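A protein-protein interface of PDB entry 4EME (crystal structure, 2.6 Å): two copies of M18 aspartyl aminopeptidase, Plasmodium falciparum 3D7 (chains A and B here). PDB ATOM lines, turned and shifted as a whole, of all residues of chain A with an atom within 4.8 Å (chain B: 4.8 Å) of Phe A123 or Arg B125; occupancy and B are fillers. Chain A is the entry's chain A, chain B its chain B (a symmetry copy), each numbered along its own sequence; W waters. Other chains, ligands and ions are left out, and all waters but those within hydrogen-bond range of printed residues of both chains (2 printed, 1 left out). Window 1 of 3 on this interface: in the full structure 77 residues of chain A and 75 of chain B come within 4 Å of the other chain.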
ATOM      1  N   TRP A 119     -15.998  10.326   6.475  1.00  0.00           N
ATOM      2  CA  TRP A 119     -14.874  11.160   6.020  1.00  0.00           C
ATOM      3  C   TRP A 119     -13.546  10.471   5.744  1.00  0.00           C
ATOM      4  O   TRP A 119     -12.877  10.842   4.778  1.00  0.00           O
ATOM      5  CB  TRP A 119     -14.701  12.453   6.841  1.00  0.00           C
ATOM      6  CG  TRP A 119     -15.961  13.257   7.026  1.00  0.00           C
ATOM      7  CD1 TRP A 119     -16.520  13.646   8.211  1.00  0.00           C
ATOM      8  CD2 TRP A 119     -16.847  13.722   5.992  1.00  0.00           C
ATOM      9  NE1 TRP A 119     -17.696  14.328   7.984  1.00  0.00           N
ATOM     10  CE2 TRP A 119     -17.920  14.393   6.630  1.00  0.00           C
ATOM     11  CE3 TRP A 119     -16.840  13.629   4.585  1.00  0.00           C
ATOM     12  CZ2 TRP A 119     -18.960  14.991   5.912  1.00  0.00           C
ATOM     13  CZ3 TRP A 119     -17.895  14.186   3.880  1.00  0.00           C
ATOM     14  CH2 TRP A 119     -18.928  14.875   4.539  1.00  0.00           C
ATOM     15  N   HIS A 120     -13.195   9.429   6.521  1.00  0.00           N
ATOM     16  CA  HIS A 120     -11.969   8.668   6.287  1.00  0.00           C
ATOM     17  C   HIS A 120     -11.960   8.053   4.885  1.00  0.00           C
ATOM     18  O   HIS A 120     -10.881   7.794   4.355  1.00  0.00           O
ATOM     19  CB  HIS A 120     -11.748   7.589   7.369  1.00  0.00           C
ATOM     20  CG  HIS A 120     -12.779   6.506   7.373  1.00  0.00           C
ATOM     21  ND1 HIS A 120     -13.935   6.614   8.130  1.00  0.00           N
ATOM     22  CD2 HIS A 120     -12.809   5.336   6.688  1.00  0.00           C
ATOM     23  CE1 HIS A 120     -14.626   5.514   7.880  1.00  0.00           C
ATOM     24  NE2 HIS A 120     -13.995   4.721   7.006  1.00  0.00           N
ATOM     25  N   THR A 121     -13.148   7.818   4.290  1.00  0.00           N
ATOM     26  CA  THR A 121     -13.277   7.252   2.941  1.00  0.00           C
ATOM     27  C   THR A 121     -12.903   8.298   1.886  1.00  0.00           C
ATOM     28  O   THR A 121     -12.502   7.922   0.789  1.00  0.00           O
ATOM     29  CB  THR A 121     -14.672   6.631   2.676  1.00  0.00           C
ATOM     30  OG1 THR A 121     -15.648   7.651   2.430  1.00  0.00           O
ATOM     31  CG2 THR A 121     -15.133   5.666   3.775  1.00  0.00           C
ATOM     32  N   TRP A 122     -12.996   9.606   2.234  1.00  0.00           N
ATOM     33  CA  TRP A 122     -12.667  10.721   1.347  1.00  0.00           C
ATOM     34  C   TRP A 122     -11.165  10.910   1.201  1.00  0.00           C
ATOM     35  O   TRP A 122     -10.720  11.598   0.276  1.00  0.00           O
ATOM     36  CB  TRP A 122     -13.331  12.012   1.831  1.00  0.00           C
ATOM     37  CG  TRP A 122     -14.786  12.078   1.491  1.00  0.00           C
ATOM     38  CD1 TRP A 122     -15.805  11.379   2.079  1.00  0.00           C
ATOM     39  CD2 TRP A 122     -15.381  12.871   0.458  1.00  0.00           C
ATOM     40  NE1 TRP A 122     -16.998  11.675   1.459  1.00  0.00           N
ATOM     41  CE2 TRP A 122     -16.770  12.603   0.471  1.00  0.00           C
ATOM     42  CE3 TRP A 122     -14.874  13.783  -0.486  1.00  0.00           C
ATOM     43  CZ2 TRP A 122     -17.653  13.210  -0.428  1.00  0.00           C
ATOM     44  CZ3 TRP A 122     -15.756  14.409  -1.353  1.00  0.00           C
ATOM     45  CH2 TRP A 122     -17.126  14.124  -1.319  1.00  0.00           C
ATOM     46  N   PHE A 123     -10.379  10.308   2.112  1.00  0.00           N
ATOM     47  CA  PHE A 123      -8.924  10.388   2.050  1.00  0.00           C
ATOM     48  C   PHE A 123      -8.399   9.518   0.930  1.00  0.00           C
ATOM     49  O   PHE A 123      -8.985   8.467   0.601  1.00  0.00           O
ATOM     50  CB  PHE A 123      -8.280   9.973   3.375  1.00  0.00           C
ATOM     51  CG  PHE A 123      -8.354  11.026   4.453  1.00  0.00           C
ATOM     52  CD1 PHE A 123      -9.567  11.346   5.053  1.00  0.00           C
ATOM     53  CD2 PHE A 123      -7.204  11.661   4.905  1.00  0.00           C
ATOM     54  CE1 PHE A 123      -9.630  12.306   6.058  1.00  0.00           C
ATOM     55  CE2 PHE A 123      -7.265  12.604   5.929  1.00  0.00           C
ATOM     56  CZ  PHE A 123      -8.475  12.921   6.500  1.00  0.00           C
ATOM     57  N   ASP A 124      -7.290   9.990   0.338  1.00  0.00           N
ATOM     58  CA  ASP A 124      -6.551   9.350  -0.745  1.00  0.00           C
ATOM     59  C   ASP A 124      -7.437   8.982  -1.930  1.00  0.00           C
ATOM     60  O   ASP A 124      -7.453   7.827  -2.373  1.00  0.00           O
ATOM     61  CB  ASP A 124      -5.735   8.165  -0.198  1.00  0.00           C
ATOM     62  CG  ASP A 124      -4.992   8.475   1.089  1.00  0.00           C
ATOM     63  OD1 ASP A 124      -4.548   9.637   1.261  1.00  0.00           O
ATOM     64  OD2 ASP A 124      -4.918   7.591   1.950  1.00  0.00           O
ATOM     65  N   ARG A 125      -8.221   9.965  -2.402  1.00  0.00           N
ATOM     66  CA  ARG A 125      -9.119   9.819  -3.549  1.00  0.00           C
ATOM     67  C   ARG A 125      -8.804  10.957  -4.514  1.00  0.00           C
ATOM     68  O   ARG A 125      -8.490  12.074  -4.082  1.00  0.00           O
ATOM     69  CB  ARG A 125     -10.610   9.930  -3.135  1.00  0.00           C
ATOM     70  CG  ARG A 125     -11.095   8.973  -2.067  1.00  0.00           C
ATOM     71  CD  ARG A 125     -11.618   7.685  -2.653  1.00  0.00           C
ATOM     72  NE  ARG A 125     -11.955   6.740  -1.596  1.00  0.00           N
ATOM     73  CZ  ARG A 125     -12.550   5.574  -1.793  1.00  0.00           C
ATOM     74  NH1 ARG A 125     -12.876   5.188  -3.018  1.00  0.00           N
ATOM     75  NH2 ARG A 125     -12.837   4.787  -0.766  1.00  0.00           N
ATOM     76  N   LEU A 155      -6.878  14.710  -0.593  1.00  0.00           N
ATOM     77  CA  LEU A 155      -6.929  14.726   0.870  1.00  0.00           C
ATOM     78  C   LEU A 155      -6.004  13.591   1.368  1.00  0.00           C
ATOM     79  O   LEU A 155      -6.385  12.422   1.361  1.00  0.00           O
ATOM     80  CB  LEU A 155      -8.392  14.593   1.353  1.00  0.00           C
ATOM     81  CG  LEU A 155      -8.672  14.519   2.858  1.00  0.00           C
ATOM     82  CD1 LEU A 155      -8.137  15.740   3.605  1.00  0.00           C
ATOM     83  CD2 LEU A 155     -10.159  14.391   3.108  1.00  0.00           C
ATOM     84  N   PRO A 156      -4.727  13.898   1.670  1.00  0.00           N
ATOM     85  CA  PRO A 156      -3.797  12.823   2.032  1.00  0.00           C
ATOM     86  C   PRO A 156      -3.867  12.318   3.477  1.00  0.00           C
ATOM     87  O   PRO A 156      -3.952  13.115   4.424  1.00  0.00           O
ATOM     88  CB  PRO A 156      -2.431  13.443   1.727  1.00  0.00           C
ATOM     89  CG  PRO A 156      -2.622  14.906   1.945  1.00  0.00           C
ATOM     90  CD  PRO A 156      -4.054  15.218   1.647  1.00  0.00           C
ATOM     91  N   SER A 157      -3.779  10.978   3.642  1.00  0.00           N
ATOM     92  CA  SER A 157      -3.729  10.354   4.960  1.00  0.00           C
ATOM     93  C   SER A 157      -2.332  10.622   5.529  1.00  0.00           C
ATOM     94  O   SER A 157      -1.419  11.001   4.797  1.00  0.00           O
ATOM     95  CB  SER A 157      -3.882   8.837   4.851  1.00  0.00           C
ATOM     96  OG  SER A 157      -5.135   8.409   4.351  1.00  0.00           O
ATOM     97  N   ILE A 174     -10.131  11.078  13.345  1.00  0.00           N
ATOM     98  CA  ILE A 174      -9.918  12.222  12.465  1.00  0.00           C
ATOM     99  C   ILE A 174     -10.433  13.468  13.139  1.00  0.00           C
ATOM    100  O   ILE A 174     -11.555  13.478  13.663  1.00  0.00           O
ATOM    101  CB  ILE A 174     -10.652  12.020  11.112  1.00  0.00           C
ATOM    102  CG1 ILE A 174     -10.236  10.730  10.431  1.00  0.00           C
ATOM    103  CG2 ILE A 174     -10.504  13.214  10.164  1.00  0.00           C
ATOM    104  CD1 ILE A 174     -11.392  10.023   9.913  1.00  0.00           C
ATOM    105  N   HIS A 179      -7.621  17.797  10.043  1.00  0.00           N
ATOM    106  CA  HIS A 179      -7.093  16.808   9.164  1.00  0.00           C
ATOM    107  C   HIS A 179      -7.831  16.763   7.887  1.00  0.00           C
ATOM    108  O   HIS A 179      -7.359  16.185   6.976  1.00  0.00           O
ATOM    109  CB  HIS A 179      -7.167  15.451   9.806  1.00  0.00           C
ATOM    110  CG  HIS A 179      -6.517  15.387  11.138  1.00  0.00           C
ATOM    111  ND1 HIS A 179      -6.959  14.567  12.138  1.00  0.00           N
ATOM    112  CD2 HIS A 179      -5.460  16.043  11.635  1.00  0.00           C
ATOM    113  CE1 HIS A 179      -6.202  14.718  13.194  1.00  0.00           C
ATOM    114  NE2 HIS A 179      -5.290  15.615  12.917  1.00  0.00           N
ATOM    115  N   ILE A 180      -9.013  17.353   7.843  1.00  0.00           N
ATOM    116  CA  ILE A 180      -9.764  17.445   6.587  1.00  0.00           C
ATOM    117  C   ILE A 180      -9.460  18.787   5.913  1.00  0.00           C
ATOM    118  O   ILE A 180     -10.173  19.782   6.091  1.00  0.00           O
ATOM    119  CB  ILE A 180     -11.266  17.091   6.701  1.00  0.00           C
ATOM    120  CG1 ILE A 180     -11.453  15.723   7.379  1.00  0.00           C
ATOM    121  CG2 ILE A 180     -11.905  17.093   5.304  1.00  0.00           C
ATOM    122  CD1 ILE A 180     -12.816  15.490   7.900  1.00  0.00           C
ATOM    123  N   GLU A 320     -21.361   0.236  -8.294  1.00  0.00           N
ATOM    124  CA  GLU A 320     -20.584   0.944  -7.274  1.00  0.00           C
ATOM    125  C   GLU A 320     -20.328   2.371  -7.720  1.00  0.00           C
ATOM    126  O   GLU A 320     -20.004   2.601  -8.884  1.00  0.00           O
ATOM    127  CB  GLU A 320     -19.274   0.203  -6.955  1.00  0.00           C
ATOM    128  CG  GLU A 320     -18.386  -0.048  -8.161  1.00  0.00           C
ATOM    129  CD  GLU A 320     -16.921  -0.338  -7.904  1.00  0.00           C
ATOM    130  OE1 GLU A 320     -16.233   0.493  -7.271  1.00  0.00           O
ATOM    131  OE2 GLU A 320     -16.445  -1.376  -8.405  1.00  0.00           O
ATOM    132  N   THR B 121      -8.297   2.529   4.026  1.00  0.00           N
ATOM    133  CA  THR B 121      -8.204   3.098   2.673  1.00  0.00           C
ATOM    134  C   THR B 121      -8.644   2.121   1.584  1.00  0.00           C
ATOM    135  O   THR B 121      -9.037   2.566   0.517  1.00  0.00           O
ATOM    136  CB  THR B 121      -6.824   3.721   2.365  1.00  0.00           C
ATOM    137  OG1 THR B 121      -5.819   2.711   2.222  1.00  0.00           O
ATOM    138  CG2 THR B 121      -6.418   4.786   3.361  1.00  0.00           C
ATOM    139  N   TRP B 122      -8.587   0.804   1.861  1.00  0.00           N
ATOM    140  CA  TRP B 122      -8.944  -0.277   0.946  1.00  0.00           C
ATOM    141  C   TRP B 122     -10.445  -0.516   0.862  1.00  0.00           C
ATOM    142  O   TRP B 122     -10.913  -1.238  -0.024  1.00  0.00           O
ATOM    143  CB  TRP B 122      -8.218  -1.562   1.341  1.00  0.00           C
ATOM    144  CG  TRP B 122      -6.784  -1.579   0.914  1.00  0.00           C
ATOM    145  CD1 TRP B 122      -5.753  -0.887   1.478  1.00  0.00           C
ATOM    146  CD2 TRP B 122      -6.207  -2.387  -0.126  1.00  0.00           C
ATOM    147  NE1 TRP B 122      -4.575  -1.184   0.832  1.00  0.00           N
ATOM    148  CE2 TRP B 122      -4.820  -2.117  -0.145  1.00  0.00           C
ATOM    149  CE3 TRP B 122      -6.728  -3.327  -1.039  1.00  0.00           C
ATOM    150  CZ2 TRP B 122      -3.943  -2.748  -1.043  1.00  0.00           C
ATOM    151  CZ3 TRP B 122      -5.863  -3.948  -1.928  1.00  0.00           C
ATOM    152  CH2 TRP B 122      -4.486  -3.655  -1.929  1.00  0.00           C
ATOM    153  N   PHE B 123     -11.201   0.080   1.790  1.00  0.00           N
ATOM    154  CA  PHE B 123     -12.649  -0.028   1.810  1.00  0.00           C
ATOM    155  C   PHE B 123     -13.209   0.854   0.743  1.00  0.00           C
ATOM    156  O   PHE B 123     -12.659   1.923   0.460  1.00  0.00           O
ATOM    157  CB  PHE B 123     -13.205   0.373   3.178  1.00  0.00           C
ATOM    158  CG  PHE B 123     -13.117  -0.723   4.216  1.00  0.00           C
ATOM    159  CD1 PHE B 123     -11.893  -1.070   4.790  1.00  0.00           C
ATOM    160  CD2 PHE B 123     -14.255  -1.408   4.625  1.00  0.00           C
ATOM    161  CE1 PHE B 123     -11.806  -2.104   5.731  1.00  0.00           C
ATOM    162  CE2 PHE B 123     -14.169  -2.433   5.581  1.00  0.00           C
ATOM    163  CZ  PHE B 123     -12.944  -2.776   6.125  1.00  0.00           C
ATOM    164  N   ASP B 124     -14.283   0.388   0.113  1.00  0.00           N
ATOM    165  CA  ASP B 124     -15.020   1.122  -0.905  1.00  0.00           C
ATOM    166  C   ASP B 124     -14.181   1.547  -2.137  1.00  0.00           C
ATOM    167  O   ASP B 124     -14.290   2.674  -2.611  1.00  0.00           O
ATOM    168  CB  ASP B 124     -15.784   2.292  -0.235  1.00  0.00           C
ATOM    169  CG  ASP B 124     -16.550   1.916   1.042  1.00  0.00           C
ATOM    170  OD1 ASP B 124     -17.047   0.766   1.133  1.00  0.00           O
ATOM    171  OD2 ASP B 124     -16.652   2.766   1.939  1.00  0.00           O
ATOM    172  N   ARG B 125     -13.337   0.628  -2.634  1.00  0.00           N
ATOM    173  CA  ARG B 125     -12.471   0.801  -3.799  1.00  0.00           C
ATOM    174  C   ARG B 125     -12.822  -0.276  -4.838  1.00  0.00           C
ATOM    175  O   ARG B 125     -13.163  -1.397  -4.455  1.00  0.00           O
ATOM    176  CB  ARG B 125     -10.982   0.636  -3.411  1.00  0.00           C
ATOM    177  CG  ARG B 125     -10.439   1.574  -2.325  1.00  0.00           C
ATOM    178  CD  ARG B 125      -9.951   2.918  -2.862  1.00  0.00           C
ATOM    179  NE  ARG B 125      -9.549   3.789  -1.759  1.00  0.00           N
ATOM    180  CZ  ARG B 125      -8.954   4.973  -1.891  1.00  0.00           C
ATOM    181  NH1 ARG B 125      -8.680   5.458  -3.097  1.00  0.00           N
ATOM    182  NH2 ARG B 125      -8.606   5.668  -0.817  1.00  0.00           N
ATOM    183  N   SER B 126     -12.715   0.055  -6.144  1.00  0.00           N
ATOM    184  CA  SER B 126     -12.938  -0.872  -7.261  1.00  0.00           C
ATOM    185  C   SER B 126     -11.706  -1.789  -7.316  1.00  0.00           C
ATOM    186  O   SER B 126     -10.643  -1.370  -7.777  1.00  0.00           O
ATOM    187  CB  SER B 126     -13.066  -0.114  -8.580  1.00  0.00           C
ATOM    188  OG  SER B 126     -13.960   0.982  -8.498  1.00  0.00           O
ATOM    189  N   LEU B 127     -11.839  -3.023  -6.801  1.00  0.00           N
ATOM    190  CA  LEU B 127     -10.725  -3.956  -6.717  1.00  0.00           C
ATOM    191  C   LEU B 127     -10.657  -5.036  -7.766  1.00  0.00           C
ATOM    192  O   LEU B 127     -11.642  -5.730  -8.037  1.00  0.00           O
ATOM    193  CB  LEU B 127     -10.569  -4.544  -5.299  1.00  0.00           C
ATOM    194  CG  LEU B 127     -10.248  -3.555  -4.175  1.00  0.00           C
ATOM    195  CD1 LEU B 127     -10.411  -4.202  -2.840  1.00  0.00           C
ATOM    196  CD2 LEU B 127      -8.834  -2.976  -4.320  1.00  0.00           C
ATOM    197  N   LEU B 153     -14.029  -7.172  -7.204  1.00  0.00           N
ATOM    198  CA  LEU B 153     -14.140  -7.230  -5.740  1.00  0.00           C
ATOM    199  C   LEU B 153     -14.369  -5.850  -5.149  1.00  0.00           C
ATOM    200  O   LEU B 153     -13.970  -4.834  -5.726  1.00  0.00           O
ATOM    201  CB  LEU B 153     -12.885  -7.877  -5.110  1.00  0.00           C
ATOM    202  CG  LEU B 153     -12.584  -9.333  -5.508  1.00  0.00           C
ATOM    203  CD1 LEU B 153     -11.109  -9.582  -5.551  1.00  0.00           C
ATOM    204  CD2 LEU B 153     -13.235 -10.315  -4.563  1.00  0.00           C
ATOM    205  N   PHE B 154     -15.037  -5.821  -3.995  1.00  0.00           N
ATOM    206  CA  PHE B 154     -15.402  -4.620  -3.262  1.00  0.00           C
ATOM    207  C   PHE B 154     -15.488  -4.963  -1.770  1.00  0.00           C
ATOM    208  O   PHE B 154     -16.164  -5.924  -1.396  1.00  0.00           O
ATOM    209  CB  PHE B 154     -16.763  -4.100  -3.771  1.00  0.00           C
ATOM    210  CG  PHE B 154     -17.073  -2.667  -3.393  1.00  0.00           C
ATOM    211  CD1 PHE B 154     -16.733  -1.617  -4.242  1.00  0.00           C
ATOM    212  CD2 PHE B 154     -17.737  -2.369  -2.207  1.00  0.00           C
ATOM    213  CE1 PHE B 154     -17.038  -0.298  -3.899  1.00  0.00           C
ATOM    214  CE2 PHE B 154     -18.013  -1.047  -1.858  1.00  0.00           C
ATOM    215  CZ  PHE B 154     -17.673  -0.027  -2.710  1.00  0.00           C
ATOM    216  N   LEU B 155     -14.767  -4.196  -0.937  1.00  0.00           N
ATOM    217  CA  LEU B 155     -14.713  -4.340   0.519  1.00  0.00           C
ATOM    218  C   LEU B 155     -15.595  -3.228   1.099  1.00  0.00           C
ATOM    219  O   LEU B 155     -15.160  -2.075   1.162  1.00  0.00           O
ATOM    220  CB  LEU B 155     -13.250  -4.241   0.998  1.00  0.00           C
ATOM    221  CG  LEU B 155     -12.992  -4.298   2.503  1.00  0.00           C
ATOM    222  CD1 LEU B 155     -13.549  -5.569   3.127  1.00  0.00           C
ATOM    223  CD2 LEU B 155     -11.519  -4.188   2.778  1.00  0.00           C
ATOM    224  N   ASP B 305      -6.219  -2.014  -6.699  1.00  0.00           N
ATOM    225  CA  ASP B 305      -7.130  -0.922  -7.039  1.00  0.00           C
ATOM    226  C   ASP B 305      -7.092  -0.748  -8.562  1.00  0.00           C
ATOM    227  O   ASP B 305      -6.007  -0.691  -9.147  1.00  0.00           O
ATOM    228  CB  ASP B 305      -6.715   0.384  -6.343  1.00  0.00           C
ATOM    229  CG  ASP B 305      -7.679   1.553  -6.492  1.00  0.00           C
ATOM    230  OD1 ASP B 305      -8.596   1.475  -7.352  1.00  0.00           O
ATOM    231  OD2 ASP B 305      -7.507   2.556  -5.767  1.00  0.00           O
ATOM    232  N   TYR B 444      -0.582  17.468   9.929  1.00  0.00           N
ATOM    233  CA  TYR B 444      -0.059  16.738  11.092  1.00  0.00           C
ATOM    234  C   TYR B 444       1.335  17.329  11.387  1.00  0.00           C
ATOM    235  O   TYR B 444       2.351  16.636  11.259  1.00  0.00           O
ATOM    236  CB  TYR B 444      -0.005  15.214  10.828  1.00  0.00           C
ATOM    237  CG  TYR B 444      -1.342  14.573  10.504  1.00  0.00           C
ATOM    238  CD1 TYR B 444      -1.836  14.560   9.198  1.00  0.00           C
ATOM    239  CD2 TYR B 444      -2.091  13.936  11.491  1.00  0.00           C
ATOM    240  CE1 TYR B 444      -3.052  13.953   8.888  1.00  0.00           C
ATOM    241  CE2 TYR B 444      -3.299  13.301  11.186  1.00  0.00           C
ATOM    242  CZ  TYR B 444      -3.773  13.308   9.881  1.00  0.00           C
ATOM    243  OH  TYR B 444      -4.960  12.686   9.563  1.00  0.00           O
ATOM    244  N   ILE B 537      -3.799   2.681  -0.080  1.00  0.00           N
ATOM    245  CA  ILE B 537      -4.025   2.127  -1.405  1.00  0.00           C
ATOM    246  C   ILE B 537      -3.721   3.191  -2.493  1.00  0.00           C
ATOM    247  O   ILE B 537      -3.578   2.835  -3.660  1.00  0.00           O
ATOM    248  CB  ILE B 537      -5.473   1.588  -1.488  1.00  0.00           C
ATOM    249  CG1 ILE B 537      -5.622   0.543  -2.615  1.00  0.00           C
ATOM    250  CG2 ILE B 537      -6.458   2.746  -1.574  1.00  0.00           C
ATOM    251  CD1 ILE B 537      -6.956  -0.038  -2.740  1.00  0.00           C
ATOM    252  N   ARG B 538      -3.660   4.478  -2.120  1.00  0.00           N
ATOM    253  CA  ARG B 538      -3.385   5.576  -3.063  1.00  0.00           C
ATOM    254  C   ARG B 538      -2.520   6.665  -2.405  1.00  0.00           C
ATOM    255  O   ARG B 538      -2.996   7.408  -1.563  1.00  0.00           O
ATOM    256  CB  ARG B 538      -4.685   6.150  -3.648  1.00  0.00           C
ATOM    257  CG  ARG B 538      -4.464   6.951  -4.907  1.00  0.00           C
ATOM    258  CD  ARG B 538      -5.754   7.137  -5.660  1.00  0.00           C
ATOM    259  NE  ARG B 538      -5.532   7.704  -6.989  1.00  0.00           N
ATOM    260  CZ  ARG B 538      -5.350   6.980  -8.089  1.00  0.00           C
ATOM    261  NH1 ARG B 538      -5.333   5.648  -8.027  1.00  0.00           N
ATOM    262  NH2 ARG B 538      -5.177   7.579  -9.260  1.00  0.00           N
HETATM  263  O   HOH W   1      -6.374  11.732  11.488  1.00  0.00           O
HETATM  264  O   HOH W   2     -11.822   4.226   1.719  1.00  0.00           O
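The backbone carbonyl oxygen of Phe B123 lies within hydrogen-bond range of the guanidinium group of Arg A125 (3.1 Å). O of Phe A123 lies within hydrogen-bond range of NH2 of Arg B125, at 3.2 Å. The side-chain hydroxyl (OG) of Ser B126 lies within hydrogen-bond range of the side-chain carboxylate (OE1) of Glu A320, 2.6 Å away. The backbone carbonyl oxygen (O) of Asp A124 is in hydrogen-bond range of the guanidinium group (NH1) of Arg B125 (2.8 Å). NH1 of Arg A125 lies within hydrogen-bond range of O of Asp B124 (2.9 Å).
NE of Arg A125 sits at hydrogen-bond distance from O of Thr A121 (2.7 Å). NE of Arg B125 lies within hydrogen-bond range of O of Thr B121, 2.6 Å away. The side-chain hydroxyl (OG1) of Thr B121 lies within hydrogen-bond range of the backbone NH (N) of Ile B537 (3.1 Å). N of Asp A124 sits at hydrogen-bond distance from O of Leu A155 (2.8 Å). The side-chain carboxylate (OD2) of Asp A124 lies within hydrogen-bond range of the side-chain hydroxyl (OG) of Ser A157, 2.5 Å away. The backbone NH (N) of Asp B124 lies within hydrogen-bond range of the backbone carbonyl oxygen (O) of Leu B155, at 2.8 Å.
Asp B124 touches Thr A121 (OD2 to CG2, 3.8 Å). Asp A124 touches Thr B121. O of Arg B538 touches CB of Asp A124 (3.2 Å). Arg B125 touches Arg A125. Ser A157 touches Thr B121 (OG to CG2, 3.97 Å). Tyr B444 touches His A179 (OH to CG, 3.5 Å). OE1 of Glu A320 touches CE1 of Phe B154, at 3.6 Å.
Phe A123 touches just one residue of chain B: Arg B125. Of chain A, only Phe A123 (3.2 Å), Asp A124 (2.8 Å) and Arg A125 (3.5 Å) come within 4 Å of Arg B125. Of the printed residues of chain B, His A179 touches Tyr B444. Printed residues of chain A within 4 Å of Arg B538: Asp A124. Printed residues of chain A within 4 Å of Thr B121: Asp A124 and Ser A157. Of the printed residues of chain A, Asp B124 touches Thr A121 (3.8 Å) and Arg A125 (2.9 Å). Of the printed residues of chain A, Ser B126 touches Glu A320. His A120 touches none of the printed residues of chain B.
Along chain B the printed residues that touch a printed residue of chain A span positions 121 to 538. Among the printed residues, no Asp or Glu carboxylate lies within 4 Å of a Lys or Arg side-chain nitrogen of the other chain.
Thr A121 touches Asp B124, and with the chains exchanged Asp A124 touches Thr B121. Phe A123 touches Arg B125, and with the chains exchanged Arg A125 touches Phe B123. Asp A124 touches Arg B125, and with the chains exchanged Arg A125 touches Asp B124. Arg B125 touches its own counterpart, Arg A125. Of the 12 pairs that touch across the chains among the printed residues, 7 have their exchanged pair printed and touching as well.
Water W1 lies within hydrogen-bond range of OH of Tyr B444 (2.6 Å) and ND1 of His A179 (3.0 Å). Water W2 lies within hydrogen-bond range of NH2 of Arg A125, O of Phe B123 and O of Thr B121.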
